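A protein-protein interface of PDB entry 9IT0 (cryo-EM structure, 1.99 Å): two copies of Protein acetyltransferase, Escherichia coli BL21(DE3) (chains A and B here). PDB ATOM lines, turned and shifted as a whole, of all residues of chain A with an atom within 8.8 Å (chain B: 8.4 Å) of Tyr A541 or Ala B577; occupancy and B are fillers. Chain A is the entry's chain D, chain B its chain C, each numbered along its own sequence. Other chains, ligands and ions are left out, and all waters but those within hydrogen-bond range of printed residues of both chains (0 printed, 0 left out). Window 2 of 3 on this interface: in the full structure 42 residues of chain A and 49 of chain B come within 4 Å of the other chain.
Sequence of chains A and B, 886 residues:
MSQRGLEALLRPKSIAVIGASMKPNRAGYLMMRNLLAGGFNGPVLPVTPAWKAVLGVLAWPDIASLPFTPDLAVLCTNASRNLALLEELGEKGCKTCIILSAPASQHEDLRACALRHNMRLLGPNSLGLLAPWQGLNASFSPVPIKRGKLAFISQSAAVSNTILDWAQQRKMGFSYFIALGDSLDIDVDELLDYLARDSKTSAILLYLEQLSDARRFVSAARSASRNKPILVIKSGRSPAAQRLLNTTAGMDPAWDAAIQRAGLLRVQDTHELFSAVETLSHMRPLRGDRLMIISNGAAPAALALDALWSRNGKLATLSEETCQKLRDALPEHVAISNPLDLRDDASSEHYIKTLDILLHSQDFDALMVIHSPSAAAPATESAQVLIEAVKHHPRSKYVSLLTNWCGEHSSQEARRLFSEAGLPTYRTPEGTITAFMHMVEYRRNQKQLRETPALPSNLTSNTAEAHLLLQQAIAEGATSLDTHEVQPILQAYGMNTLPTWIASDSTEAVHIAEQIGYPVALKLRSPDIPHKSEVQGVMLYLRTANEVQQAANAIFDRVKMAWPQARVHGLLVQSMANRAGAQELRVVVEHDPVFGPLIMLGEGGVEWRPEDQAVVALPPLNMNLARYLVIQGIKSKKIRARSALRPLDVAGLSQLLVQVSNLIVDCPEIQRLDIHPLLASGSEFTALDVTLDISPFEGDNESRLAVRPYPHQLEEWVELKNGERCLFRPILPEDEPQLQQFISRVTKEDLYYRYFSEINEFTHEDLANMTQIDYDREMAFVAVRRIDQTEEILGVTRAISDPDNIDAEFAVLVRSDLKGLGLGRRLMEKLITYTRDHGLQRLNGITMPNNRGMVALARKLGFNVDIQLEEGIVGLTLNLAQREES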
ATOM      1  N   TYR A 518      28.790 -17.433  17.394  1.00  0.00           N
ATOM      2  CA  TYR A 518      27.748 -17.044  18.330  1.00  0.00           C
ATOM      3  C   TYR A 518      27.017 -15.851  17.752  1.00  0.00           C
ATOM      4  O   TYR A 518      27.486 -15.234  16.785  1.00  0.00           O
ATOM      5  CB  TYR A 518      28.330 -16.690  19.707  1.00  0.00           C
ATOM      6  CG  TYR A 518      28.249 -17.805  20.725  1.00  0.00           C
ATOM      7  CD1 TYR A 518      29.250 -18.765  20.806  1.00  0.00           C
ATOM      8  CD2 TYR A 518      27.183 -17.896  21.609  1.00  0.00           C
ATOM      9  CE1 TYR A 518      29.190 -19.786  21.731  1.00  0.00           C
ATOM     10  CE2 TYR A 518      27.114 -18.916  22.541  1.00  0.00           C
ATOM     11  CZ  TYR A 518      28.121 -19.858  22.597  1.00  0.00           C
ATOM     12  OH  TYR A 518      28.061 -20.876  23.521  1.00  0.00           O
ATOM     13  N   PRO A 519      25.855 -15.497  18.300  1.00  0.00           N
ATOM     14  CA  PRO A 519      25.164 -14.292  17.830  1.00  0.00           C
ATOM     15  C   PRO A 519      26.038 -13.060  18.007  1.00  0.00           C
ATOM     16  O   PRO A 519      26.734 -12.911  19.013  1.00  0.00           O
ATOM     17  CB  PRO A 519      23.909 -14.228  18.707  1.00  0.00           C
ATOM     18  CG  PRO A 519      23.723 -15.602  19.229  1.00  0.00           C
ATOM     19  CD  PRO A 519      25.097 -16.190  19.356  1.00  0.00           C
ATOM     20  N   VAL A 538      16.624  -8.322  15.332  1.00  0.00           N
ATOM     21  CA  VAL A 538      17.219  -8.396  16.660  1.00  0.00           C
ATOM     22  C   VAL A 538      17.793  -9.795  16.841  1.00  0.00           C
ATOM     23  O   VAL A 538      17.162 -10.800  16.512  1.00  0.00           O
ATOM     24  CB  VAL A 538      16.206  -8.072  17.780  1.00  0.00           C
ATOM     25  CG1 VAL A 538      15.209  -9.209  17.959  1.00  0.00           C
ATOM     26  CG2 VAL A 538      16.934  -7.782  19.084  1.00  0.00           C
ATOM     27  N   MET A 539      19.012  -9.848  17.368  1.00  0.00           N
ATOM     28  CA  MET A 539      19.720 -11.101  17.581  1.00  0.00           C
ATOM     29  C   MET A 539      19.327 -11.690  18.927  1.00  0.00           C
ATOM     30  O   MET A 539      19.925 -11.366  19.959  1.00  0.00           O
ATOM     31  CB  MET A 539      21.236 -10.896  17.511  1.00  0.00           C
ATOM     32  CG  MET A 539      21.730 -10.440  16.145  1.00  0.00           C
ATOM     33  SD  MET A 539      21.233  -8.758  15.726  1.00  0.00           S
ATOM     34  CE  MET A 539      21.398  -8.792  13.942  1.00  0.00           C
ATOM     35  N   LEU A 540      18.315 -12.557  18.904  1.00  0.00           N
ATOM     36  CA  LEU A 540      17.830 -13.224  20.111  1.00  0.00           C
ATOM     37  C   LEU A 540      17.447 -14.644  19.701  1.00  0.00           C
ATOM     38  O   LEU A 540      16.410 -14.851  19.063  1.00  0.00           O
ATOM     39  CB  LEU A 540      16.656 -12.464  20.715  1.00  0.00           C
ATOM     40  CG  LEU A 540      15.907 -13.098  21.890  1.00  0.00           C
ATOM     41  CD1 LEU A 540      15.691 -12.063  22.987  1.00  0.00           C
ATOM     42  CD2 LEU A 540      14.580 -13.691  21.444  1.00  0.00           C
ATOM     43  N   TYR A 541      18.293 -15.606  20.062  1.00  0.00           N
ATOM     44  CA  TYR A 541      18.134 -17.011  19.683  1.00  0.00           C
ATOM     45  C   TYR A 541      18.460 -17.238  18.204  1.00  0.00           C
ATOM     46  O   TYR A 541      17.924 -18.131  17.547  1.00  0.00           O
ATOM     47  CB  TYR A 541      16.730 -17.521  20.016  1.00  0.00           C
ATOM     48  CG  TYR A 541      16.689 -19.021  20.200  1.00  0.00           C
ATOM     49  CD1 TYR A 541      17.001 -19.595  21.422  1.00  0.00           C
ATOM     50  CD2 TYR A 541      16.339 -19.862  19.152  1.00  0.00           C
ATOM     51  CE1 TYR A 541      16.973 -20.965  21.595  1.00  0.00           C
ATOM     52  CE2 TYR A 541      16.306 -21.234  19.316  1.00  0.00           C
ATOM     53  CZ  TYR A 541      16.623 -21.780  20.541  1.00  0.00           C
ATOM     54  OH  TYR A 541      16.593 -23.143  20.716  1.00  0.00           O
ATOM     55  N   LEU A 542      19.350 -16.401  17.682  1.00  0.00           N
ATOM     56  CA  LEU A 542      20.036 -16.696  16.424  1.00  0.00           C
ATOM     57  C   LEU A 542      21.423 -17.270  16.698  1.00  0.00           C
ATOM     58  O   LEU A 542      22.441 -16.748  16.245  1.00  0.00           O
ATOM     59  CB  LEU A 542      20.109 -15.443  15.561  1.00  0.00           C
ATOM     60  CG  LEU A 542      18.768 -14.988  14.973  1.00  0.00           C
ATOM     61  CD1 LEU A 542      18.113 -13.936  15.851  1.00  0.00           C
ATOM     62  CD2 LEU A 542      18.943 -14.459  13.556  1.00  0.00           C
ATOM     63  N   ARG A 543      21.464 -18.369  17.456  1.00  0.00           N
ATOM     64  CA  ARG A 543      22.707 -18.851  18.050  1.00  0.00           C
ATOM     65  C   ARG A 543      23.407 -19.914  17.212  1.00  0.00           C
ATOM     66  O   ARG A 543      24.531 -19.700  16.748  1.00  0.00           O
ATOM     67  CB  ARG A 543      22.427 -19.426  19.441  1.00  0.00           C
ATOM     68  CG  ARG A 543      23.676 -19.642  20.275  1.00  0.00           C
ATOM     69  CD  ARG A 543      23.387 -20.516  21.479  1.00  0.00           C
ATOM     70  NE  ARG A 543      22.236 -20.057  22.246  1.00  0.00           N
ATOM     71  CZ  ARG A 543      21.665 -20.754  23.218  1.00  0.00           C
ATOM     72  NH1 ARG A 543      22.108 -21.952  23.564  1.00  0.00           N
ATOM     73  NH2 ARG A 543      20.618 -20.240  23.856  1.00  0.00           N
ATOM     74  N   THR A 544      22.762 -21.058  17.008  1.00  0.00           N
ATOM     75  CA  THR A 544      23.452 -22.223  16.478  1.00  0.00           C
ATOM     76  C   THR A 544      23.916 -21.973  15.049  1.00  0.00           C
ATOM     77  O   THR A 544      23.309 -21.202  14.300  1.00  0.00           O
ATOM     78  CB  THR A 544      22.549 -23.457  16.525  1.00  0.00           C
ATOM     79  OG1 THR A 544      21.426 -23.273  15.655  1.00  0.00           O
ATOM     80  CG2 THR A 544      22.049 -23.698  17.943  1.00  0.00           C
ATOM     81  N   ASN A 546      23.631 -23.798  12.557  1.00  0.00           N
ATOM     82  CA  ASN A 546      22.466 -24.032  11.709  1.00  0.00           C
ATOM     83  C   ASN A 546      21.502 -22.855  11.787  1.00  0.00           C
ATOM     84  O   ASN A 546      20.972 -22.399  10.764  1.00  0.00           O
ATOM     85  CB  ASN A 546      21.769 -25.330  12.122  1.00  0.00           C
ATOM     86  CG  ASN A 546      21.493 -25.396  13.612  1.00  0.00           C
ATOM     87  OD1 ASN A 546      20.570 -24.753  14.113  1.00  0.00           O
ATOM     88  ND2 ASN A 546      22.297 -26.171  14.330  1.00  0.00           N
ATOM     89  N   GLU A 547      21.261 -22.348  13.000  1.00  0.00           N
ATOM     90  CA  GLU A 547      20.430 -21.160  13.145  1.00  0.00           C
ATOM     91  C   GLU A 547      21.044 -19.980  12.410  1.00  0.00           C
ATOM     92  O   GLU A 547      20.357 -19.286  11.655  1.00  0.00           O
ATOM     93  CB  GLU A 547      20.236 -20.817  14.622  1.00  0.00           C
ATOM     94  CG  GLU A 547      19.067 -21.532  15.284  1.00  0.00           C
ATOM     95  CD  GLU A 547      17.734 -20.867  14.993  1.00  0.00           C
ATOM     96  OE1 GLU A 547      17.716 -19.855  14.262  1.00  0.00           O
ATOM     97  OE2 GLU A 547      16.703 -21.359  15.497  1.00  0.00           O
ATOM     98  N   VAL A 548      22.344 -19.747  12.600  1.00  0.00           N
ATOM     99  CA  VAL A 548      22.994 -18.648  11.895  1.00  0.00           C
ATOM    100  C   VAL A 548      22.767 -18.789  10.398  1.00  0.00           C
ATOM    101  O   VAL A 548      22.198 -17.900   9.758  1.00  0.00           O
ATOM    102  CB  VAL A 548      24.495 -18.599  12.239  1.00  0.00           C
ATOM    103  CG1 VAL A 548      25.241 -17.700  11.258  1.00  0.00           C
ATOM    104  CG2 VAL A 548      24.698 -18.114  13.664  1.00  0.00           C
ATOM    105  N   ALA A 551      18.645 -18.719   9.419  1.00  0.00           N
ATOM    106  CA  ALA A 551      17.997 -17.457   9.745  1.00  0.00           C
ATOM    107  C   ALA A 551      18.648 -16.296   9.012  1.00  0.00           C
ATOM    108  O   ALA A 551      17.950 -15.434   8.470  1.00  0.00           O
ATOM    109  CB  ALA A 551      18.036 -17.228  11.257  1.00  0.00           C
ATOM    110  N   MET A 576      27.772  -8.985  20.042  1.00  0.00           N
ATOM    111  CA  MET A 576      26.529  -9.126  20.788  1.00  0.00           C
ATOM    112  C   MET A 576      26.649  -8.510  22.176  1.00  0.00           C
ATOM    113  O   MET A 576      27.680  -8.634  22.842  1.00  0.00           O
ATOM    114  CB  MET A 576      26.166 -10.608  20.900  1.00  0.00           C
ATOM    115  CG  MET A 576      24.878 -10.897  21.662  1.00  0.00           C
ATOM    116  SD  MET A 576      24.288 -12.600  21.598  1.00  0.00           S
ATOM    117  CE  MET A 576      22.906 -12.533  22.739  1.00  0.00           C
ATOM    118  N   ASN A 578      24.460  -8.444  25.833  1.00  0.00           N
ATOM    119  CA  ASN A 578      23.348  -9.009  26.581  1.00  0.00           C
ATOM    120  C   ASN A 578      22.478  -7.896  27.151  1.00  0.00           C
ATOM    121  O   ASN A 578      22.958  -7.009  27.862  1.00  0.00           O
ATOM    122  CB  ASN A 578      23.864  -9.902  27.710  1.00  0.00           C
ATOM    123  CG  ASN A 578      22.751 -10.664  28.406  1.00  0.00           C
ATOM    124  OD1 ASN A 578      21.660 -10.823  27.861  1.00  0.00           O
ATOM    125  ND2 ASN A 578      23.024 -11.138  29.617  1.00  0.00           N
ATOM    126  N   ALA A 580      18.860  -8.956  27.975  1.00  0.00           N
ATOM    127  CA  ALA A 580      17.862  -9.643  28.785  1.00  0.00           C
ATOM    128  C   ALA A 580      18.246  -9.628  30.258  1.00  0.00           C
ATOM    129  O   ALA A 580      17.444  -9.239  31.114  1.00  0.00           O
ATOM    130  CB  ALA A 580      17.694 -11.078  28.289  1.00  0.00           C
ATOM    131  N   LEU B 498       8.097 -25.305  31.498  1.00  0.00           N
ATOM    132  CA  LEU B 498       9.438 -25.537  30.972  1.00  0.00           C
ATOM    133  C   LEU B 498      10.042 -26.778  31.623  1.00  0.00           C
ATOM    134  O   LEU B 498       9.986 -26.913  32.850  1.00  0.00           O
ATOM    135  CB  LEU B 498      10.332 -24.321  31.226  1.00  0.00           C
ATOM    136  CG  LEU B 498      11.391 -23.959  30.177  1.00  0.00           C
ATOM    137  CD1 LEU B 498      10.857 -24.047  28.751  1.00  0.00           C
ATOM    138  CD2 LEU B 498      11.946 -22.568  30.448  1.00  0.00           C
ATOM    139  N   GLY B 517      21.730 -27.116  25.931  1.00  0.00           N
ATOM    140  CA  GLY B 517      22.310 -25.808  25.696  1.00  0.00           C
ATOM    141  C   GLY B 517      23.063 -25.282  26.901  1.00  0.00           C
ATOM    142  O   GLY B 517      22.542 -25.300  28.020  1.00  0.00           O
ATOM    143  N   TYR B 518      24.291 -24.810  26.687  1.00  0.00           N
ATOM    144  CA  TYR B 518      25.103 -24.320  27.800  1.00  0.00           C
ATOM    145  C   TYR B 518      24.470 -23.156  28.549  1.00  0.00           C
ATOM    146  O   TYR B 518      24.587 -23.119  29.786  1.00  0.00           O
ATOM    147  CB  TYR B 518      26.507 -23.967  27.299  1.00  0.00           C
ATOM    148  CG  TYR B 518      27.317 -25.187  26.932  1.00  0.00           C
ATOM    149  CD1 TYR B 518      28.029 -25.879  27.903  1.00  0.00           C
ATOM    150  CD2 TYR B 518      27.366 -25.653  25.626  1.00  0.00           C
ATOM    151  CE1 TYR B 518      28.770 -26.998  27.586  1.00  0.00           C
ATOM    152  CE2 TYR B 518      28.108 -26.775  25.298  1.00  0.00           C
ATOM    153  CZ  TYR B 518      28.807 -27.441  26.283  1.00  0.00           C
ATOM    154  OH  TYR B 518      29.547 -28.558  25.967  1.00  0.00           O
ATOM    155  N   PRO B 519      23.829 -22.177  27.907  1.00  0.00           N
ATOM    156  CA  PRO B 519      23.136 -21.146  28.698  1.00  0.00           C
ATOM    157  C   PRO B 519      22.005 -21.774  29.501  1.00  0.00           C
ATOM    158  O   PRO B 519      20.992 -22.200  28.943  1.00  0.00           O
ATOM    159  CB  PRO B 519      22.620 -20.163  27.640  1.00  0.00           C
ATOM    160  CG  PRO B 519      22.667 -20.899  26.354  1.00  0.00           C
ATOM    161  CD  PRO B 519      23.792 -21.875  26.466  1.00  0.00           C
ATOM    162  N   VAL B 520      22.188 -21.824  30.823  1.00  0.00           N
ATOM    163  CA  VAL B 520      21.289 -22.528  31.727  1.00  0.00           C
ATOM    164  C   VAL B 520      21.167 -21.738  33.022  1.00  0.00           C
ATOM    165  O   VAL B 520      21.864 -20.746  33.246  1.00  0.00           O
ATOM    166  CB  VAL B 520      21.764 -23.968  32.035  1.00  0.00           C
ATOM    167  CG1 VAL B 520      22.026 -24.749  30.756  1.00  0.00           C
ATOM    168  CG2 VAL B 520      23.010 -23.942  32.909  1.00  0.00           C
ATOM    169  N   ALA B 521      20.263 -22.202  33.882  1.00  0.00           N
ATOM    170  CA  ALA B 521      20.045 -21.628  35.202  1.00  0.00           C
ATOM    171  C   ALA B 521      20.150 -22.731  36.246  1.00  0.00           C
ATOM    172  O   ALA B 521      19.696 -23.856  36.012  1.00  0.00           O
ATOM    173  CB  ALA B 521      18.678 -20.944  35.289  1.00  0.00           C
ATOM    174  N   LEU B 540      21.234 -17.190  36.844  1.00  0.00           N
ATOM    175  CA  LEU B 540      20.925 -17.603  35.486  1.00  0.00           C
ATOM    176  C   LEU B 540      21.916 -16.980  34.511  1.00  0.00           C
ATOM    177  O   LEU B 540      22.803 -16.210  34.894  1.00  0.00           O
ATOM    178  CB  LEU B 540      19.481 -17.228  35.132  1.00  0.00           C
ATOM    179  CG  LEU B 540      19.037 -15.796  35.446  1.00  0.00           C
ATOM    180  CD1 LEU B 540      17.962 -15.348  34.475  1.00  0.00           C
ATOM    181  CD2 LEU B 540      18.516 -15.694  36.872  1.00  0.00           C
ATOM    182  N   TYR B 541      21.761 -17.332  33.233  1.00  0.00           N
ATOM    183  CA  TYR B 541      22.620 -16.849  32.151  1.00  0.00           C
ATOM    184  C   TYR B 541      24.086 -17.219  32.406  1.00  0.00           C
ATOM    185  O   TYR B 541      24.953 -16.368  32.614  1.00  0.00           O
ATOM    186  CB  TYR B 541      22.456 -15.337  31.954  1.00  0.00           C
ATOM    187  CG  TYR B 541      21.258 -14.961  31.114  1.00  0.00           C
ATOM    188  CD1 TYR B 541      21.292 -15.079  29.732  1.00  0.00           C
ATOM    189  CD2 TYR B 541      20.100 -14.469  31.701  1.00  0.00           C
ATOM    190  CE1 TYR B 541      20.203 -14.734  28.958  1.00  0.00           C
ATOM    191  CE2 TYR B 541      19.004 -14.119  30.933  1.00  0.00           C
ATOM    192  CZ  TYR B 541      19.062 -14.254  29.562  1.00  0.00           C
ATOM    193  OH  TYR B 541      17.976 -13.907  28.792  1.00  0.00           O
ATOM    194  N   GLN B 574      18.034 -26.128  34.224  1.00  0.00           N
ATOM    195  CA  GLN B 574      17.147 -25.939  33.088  1.00  0.00           C
ATOM    196  C   GLN B 574      17.841 -25.045  32.074  1.00  0.00           C
ATOM    197  O   GLN B 574      18.513 -24.075  32.437  1.00  0.00           O
ATOM    198  CB  GLN B 574      15.810 -25.314  33.502  1.00  0.00           C
ATOM    199  CG  GLN B 574      15.947 -24.079  34.379  1.00  0.00           C
ATOM    200  CD  GLN B 574      14.960 -24.061  35.526  1.00  0.00           C
ATOM    201  OE1 GLN B 574      13.780 -24.363  35.351  1.00  0.00           O
ATOM    202  NE2 GLN B 574      15.439 -23.705  36.712  1.00  0.00           N
ATOM    203  N   SER B 575      17.676 -25.380  30.798  1.00  0.00           N
ATOM    204  CA  SER B 575      18.228 -24.548  29.739  1.00  0.00           C
ATOM    205  C   SER B 575      17.400 -23.283  29.585  1.00  0.00           C
ATOM    206  O   SER B 575      16.188 -23.345  29.355  1.00  0.00           O
ATOM    207  CB  SER B 575      18.263 -25.312  28.418  1.00  0.00           C
ATOM    208  OG  SER B 575      18.874 -26.574  28.582  1.00  0.00           O
ATOM    209  N   MET B 576      18.055 -22.136  29.710  1.00  0.00           N
ATOM    210  CA  MET B 576      17.439 -20.847  29.416  1.00  0.00           C
ATOM    211  C   MET B 576      18.241 -20.251  28.261  1.00  0.00           C
ATOM    212  O   MET B 576      19.390 -19.840  28.418  1.00  0.00           O
ATOM    213  CB  MET B 576      17.381 -19.932  30.668  1.00  0.00           C
ATOM    214  CG  MET B 576      18.605 -19.057  30.993  1.00  0.00           C
ATOM    215  SD  MET B 576      18.192 -17.523  31.853  1.00  0.00           S
ATOM    216  CE  MET B 576      16.933 -16.811  30.796  1.00  0.00           C
ATOM    217  N   ALA B 577      17.654 -20.296  27.072  1.00  0.00           N
ATOM    218  CA  ALA B 577      18.194 -19.553  25.948  1.00  0.00           C
ATOM    219  C   ALA B 577      17.898 -18.074  26.144  1.00  0.00           C
ATOM    220  O   ALA B 577      16.933 -17.708  26.817  1.00  0.00           O
ATOM    221  CB  ALA B 577      17.597 -20.049  24.634  1.00  0.00           C
ATOM    222  N   ASN B 578      18.737 -17.222  25.562  1.00  0.00           N
ATOM    223  CA  ASN B 578      18.557 -15.787  25.734  1.00  0.00           C
ATOM    224  C   ASN B 578      17.171 -15.364  25.264  1.00  0.00           C
ATOM    225  O   ASN B 578      16.888 -15.382  24.062  1.00  0.00           O
ATOM    226  CB  ASN B 578      19.632 -15.015  24.968  1.00  0.00           C
ATOM    227  CG  ASN B 578      19.651 -13.541  25.320  1.00  0.00           C
ATOM    228  OD1 ASN B 578      19.467 -13.165  26.479  1.00  0.00           O
ATOM    229  ND2 ASN B 578      19.867 -12.696  24.318  1.00  0.00           N
ATOM    230  N   ARG B 579      16.300 -14.986  26.198  1.00  0.00           N
ATOM    231  CA  ARG B 579      14.993 -14.451  25.822  1.00  0.00           C
ATOM    232  C   ARG B 579      14.504 -13.515  26.916  1.00  0.00           C
ATOM    233  O   ARG B 579      14.303 -13.937  28.060  1.00  0.00           O
ATOM    234  CB  ARG B 579      13.980 -15.587  25.536  1.00  0.00           C
ATOM    235  CG  ARG B 579      13.284 -16.274  26.730  1.00  0.00           C
ATOM    236  CD  ARG B 579      13.923 -17.604  27.104  1.00  0.00           C
ATOM    237  NE  ARG B 579      14.086 -18.492  25.959  1.00  0.00           N
ATOM    238  CZ  ARG B 579      13.089 -19.095  25.326  1.00  0.00           C
ATOM    239  NH1 ARG B 579      11.831 -18.937  25.706  1.00  0.00           N
ATOM    240  NH2 ARG B 579      13.360 -19.877  24.284  1.00  0.00           N
ATOM    241  N   ALA B 580      14.388 -12.233  26.581  1.00  0.00           N
ATOM    242  CA  ALA B 580      13.658 -11.273  27.400  1.00  0.00           C
ATOM    243  C   ALA B 580      12.771 -10.422  26.503  1.00  0.00           C
ATOM    244  O   ALA B 580      11.810  -9.805  26.973  1.00  0.00           O
ATOM    245  CB  ALA B 580      14.610 -10.389  28.204  1.00  0.00           C
ATOM    246  N   LEU B 679       5.735 -16.609  30.280  1.00  0.00           N
ATOM    247  CA  LEU B 679       6.266 -16.196  28.987  1.00  0.00           C
ATOM    248  C   LEU B 679       5.140 -16.148  27.963  1.00  0.00           C
ATOM    249  O   LEU B 679       4.449 -17.149  27.744  1.00  0.00           O
ATOM    250  CB  LEU B 679       7.364 -17.150  28.521  1.00  0.00           C
ATOM    251  CG  LEU B 679       8.797 -16.665  28.739  1.00  0.00           C
ATOM    252  CD1 LEU B 679       8.996 -16.213  30.179  1.00  0.00           C
ATOM    253  CD2 LEU B 679       9.793 -17.749  28.350  1.00  0.00           C
ATOM    254  N   LEU B 688       7.616 -20.662  33.571  1.00  0.00           N
ATOM    255  CA  LEU B 688       9.037 -20.860  33.838  1.00  0.00           C
ATOM    256  C   LEU B 688       9.303 -21.340  35.260  1.00  0.00           C
ATOM    257  O   LEU B 688       9.914 -22.394  35.454  1.00  0.00           O
ATOM    258  CB  LEU B 688       9.799 -19.556  33.576  1.00  0.00           C
ATOM    259  CG  LEU B 688      10.713 -19.569  32.350  1.00  0.00           C
ATOM    260  CD1 LEU B 688       9.893 -19.668  31.075  1.00  0.00           C
ATOM    261  CD2 LEU B 688      11.596 -18.329  32.328  1.00  0.00           C
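The side-chain amide oxygen (OD1) of Asn A578 lies close to the side-chain amide oxygen (OD1) of Asn B578 (3.5 Å).
The backbone NH of Met B576 sits at hydrogen-bond distance from the backbone carbonyl oxygen of Pro B519 (3.0 Å). O of Val B520 lies within hydrogen-bond range of N of Tyr B541. OD1 of Asn B578 is in hydrogen-bond range of OH of Tyr B541 (2.9 Å). The side-chain hydroxyl (OH) of Tyr B541 sits at hydrogen-bond distance from the backbone NH (N) of Arg B579 (3.3 Å). The backbone carbonyl oxygen (O) of Ala B577 lies close to the guanidinium group (NE) of Arg B579, at 3.1 Å. N of Ala A580 sits at hydrogen-bond distance from OD1 of Asn A578 (3.4 Å).
Among the printed residues, merely in contact across the chains: Leu A540 with Asn B578 (3.3 Å), Leu A540 with Arg B579 (3.8 Å), Leu A540 with Ala B580 (3.8 Å), Tyr A541 with Ala B577 (3.2 Å), Arg A543 with Pro B519 (3.0 Å), Arg A543 with Ala B577 (3.1 Å), Arg A543 with Asn B578 (3.9 Å), Met A576 with Asn B578 (3.4 Å), Ala A580 with Tyr B541 (2.9 Å), Ala A580 with Asn B578 (3.3 Å) and Ala A580 with Ala B580 (3.2 Å).
Printed residues of chain B within 4 Å of Ala A580: Tyr B541 (2.9 Å), Asn B578 (3.3 Å) and Ala B580 (3.2 Å). Printed residues of chain A within 4 Å of Arg B579: Leu A540 (3.8 Å). Printed residues of chain A within 4 Å of Pro B519: Arg A543. Of the printed residues of chain B, Asn A578 touches Asn B578. Gln B574 touches none of the printed residues of chain A. The nearest residue of chain B that does not touch Tyr A541 is Asn B578 (4.2 Å). The nearest printed residue of chain A that does not touch Pro B519 is Tyr A518 (5.3 Å).
Of the 16 printed residues of chain A, 6 touch a printed residue of chain B. Hydrophobic or aromatic side chains of chain A within 4 Å of the printed part of chain B: Leu A540, Tyr A541, Met A576 and Ala A580. Along chain A the printed residues that touch a printed residue of chain B span positions 540 to 580. Among the printed residues, no Asp or Glu carboxylate lies within 4 Å of a Lys or Arg side-chain nitrogen of the other chain.
Leu A540 touches Asn B578, but with the chains exchanged Asn A578 does not touch Leu B540 (7.3 Å). Met A576 touches Asn B578, but with the chains exchanged Asn A578 does not touch Met B576 (8.2 Å). Ala A580 touches Tyr B541, but with the chains exchanged Tyr A541 does not touch Ala B580 (8.3 Å). Ala A580 touches Asn B578, but with the chains exchanged Asn A578 does not touch Ala B580 (7.1 Å). 7 positions are printed for both chains. Of the 12 pairs that touch across the chains among the printed residues, 2 have their exchanged pair printed and touching as well.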
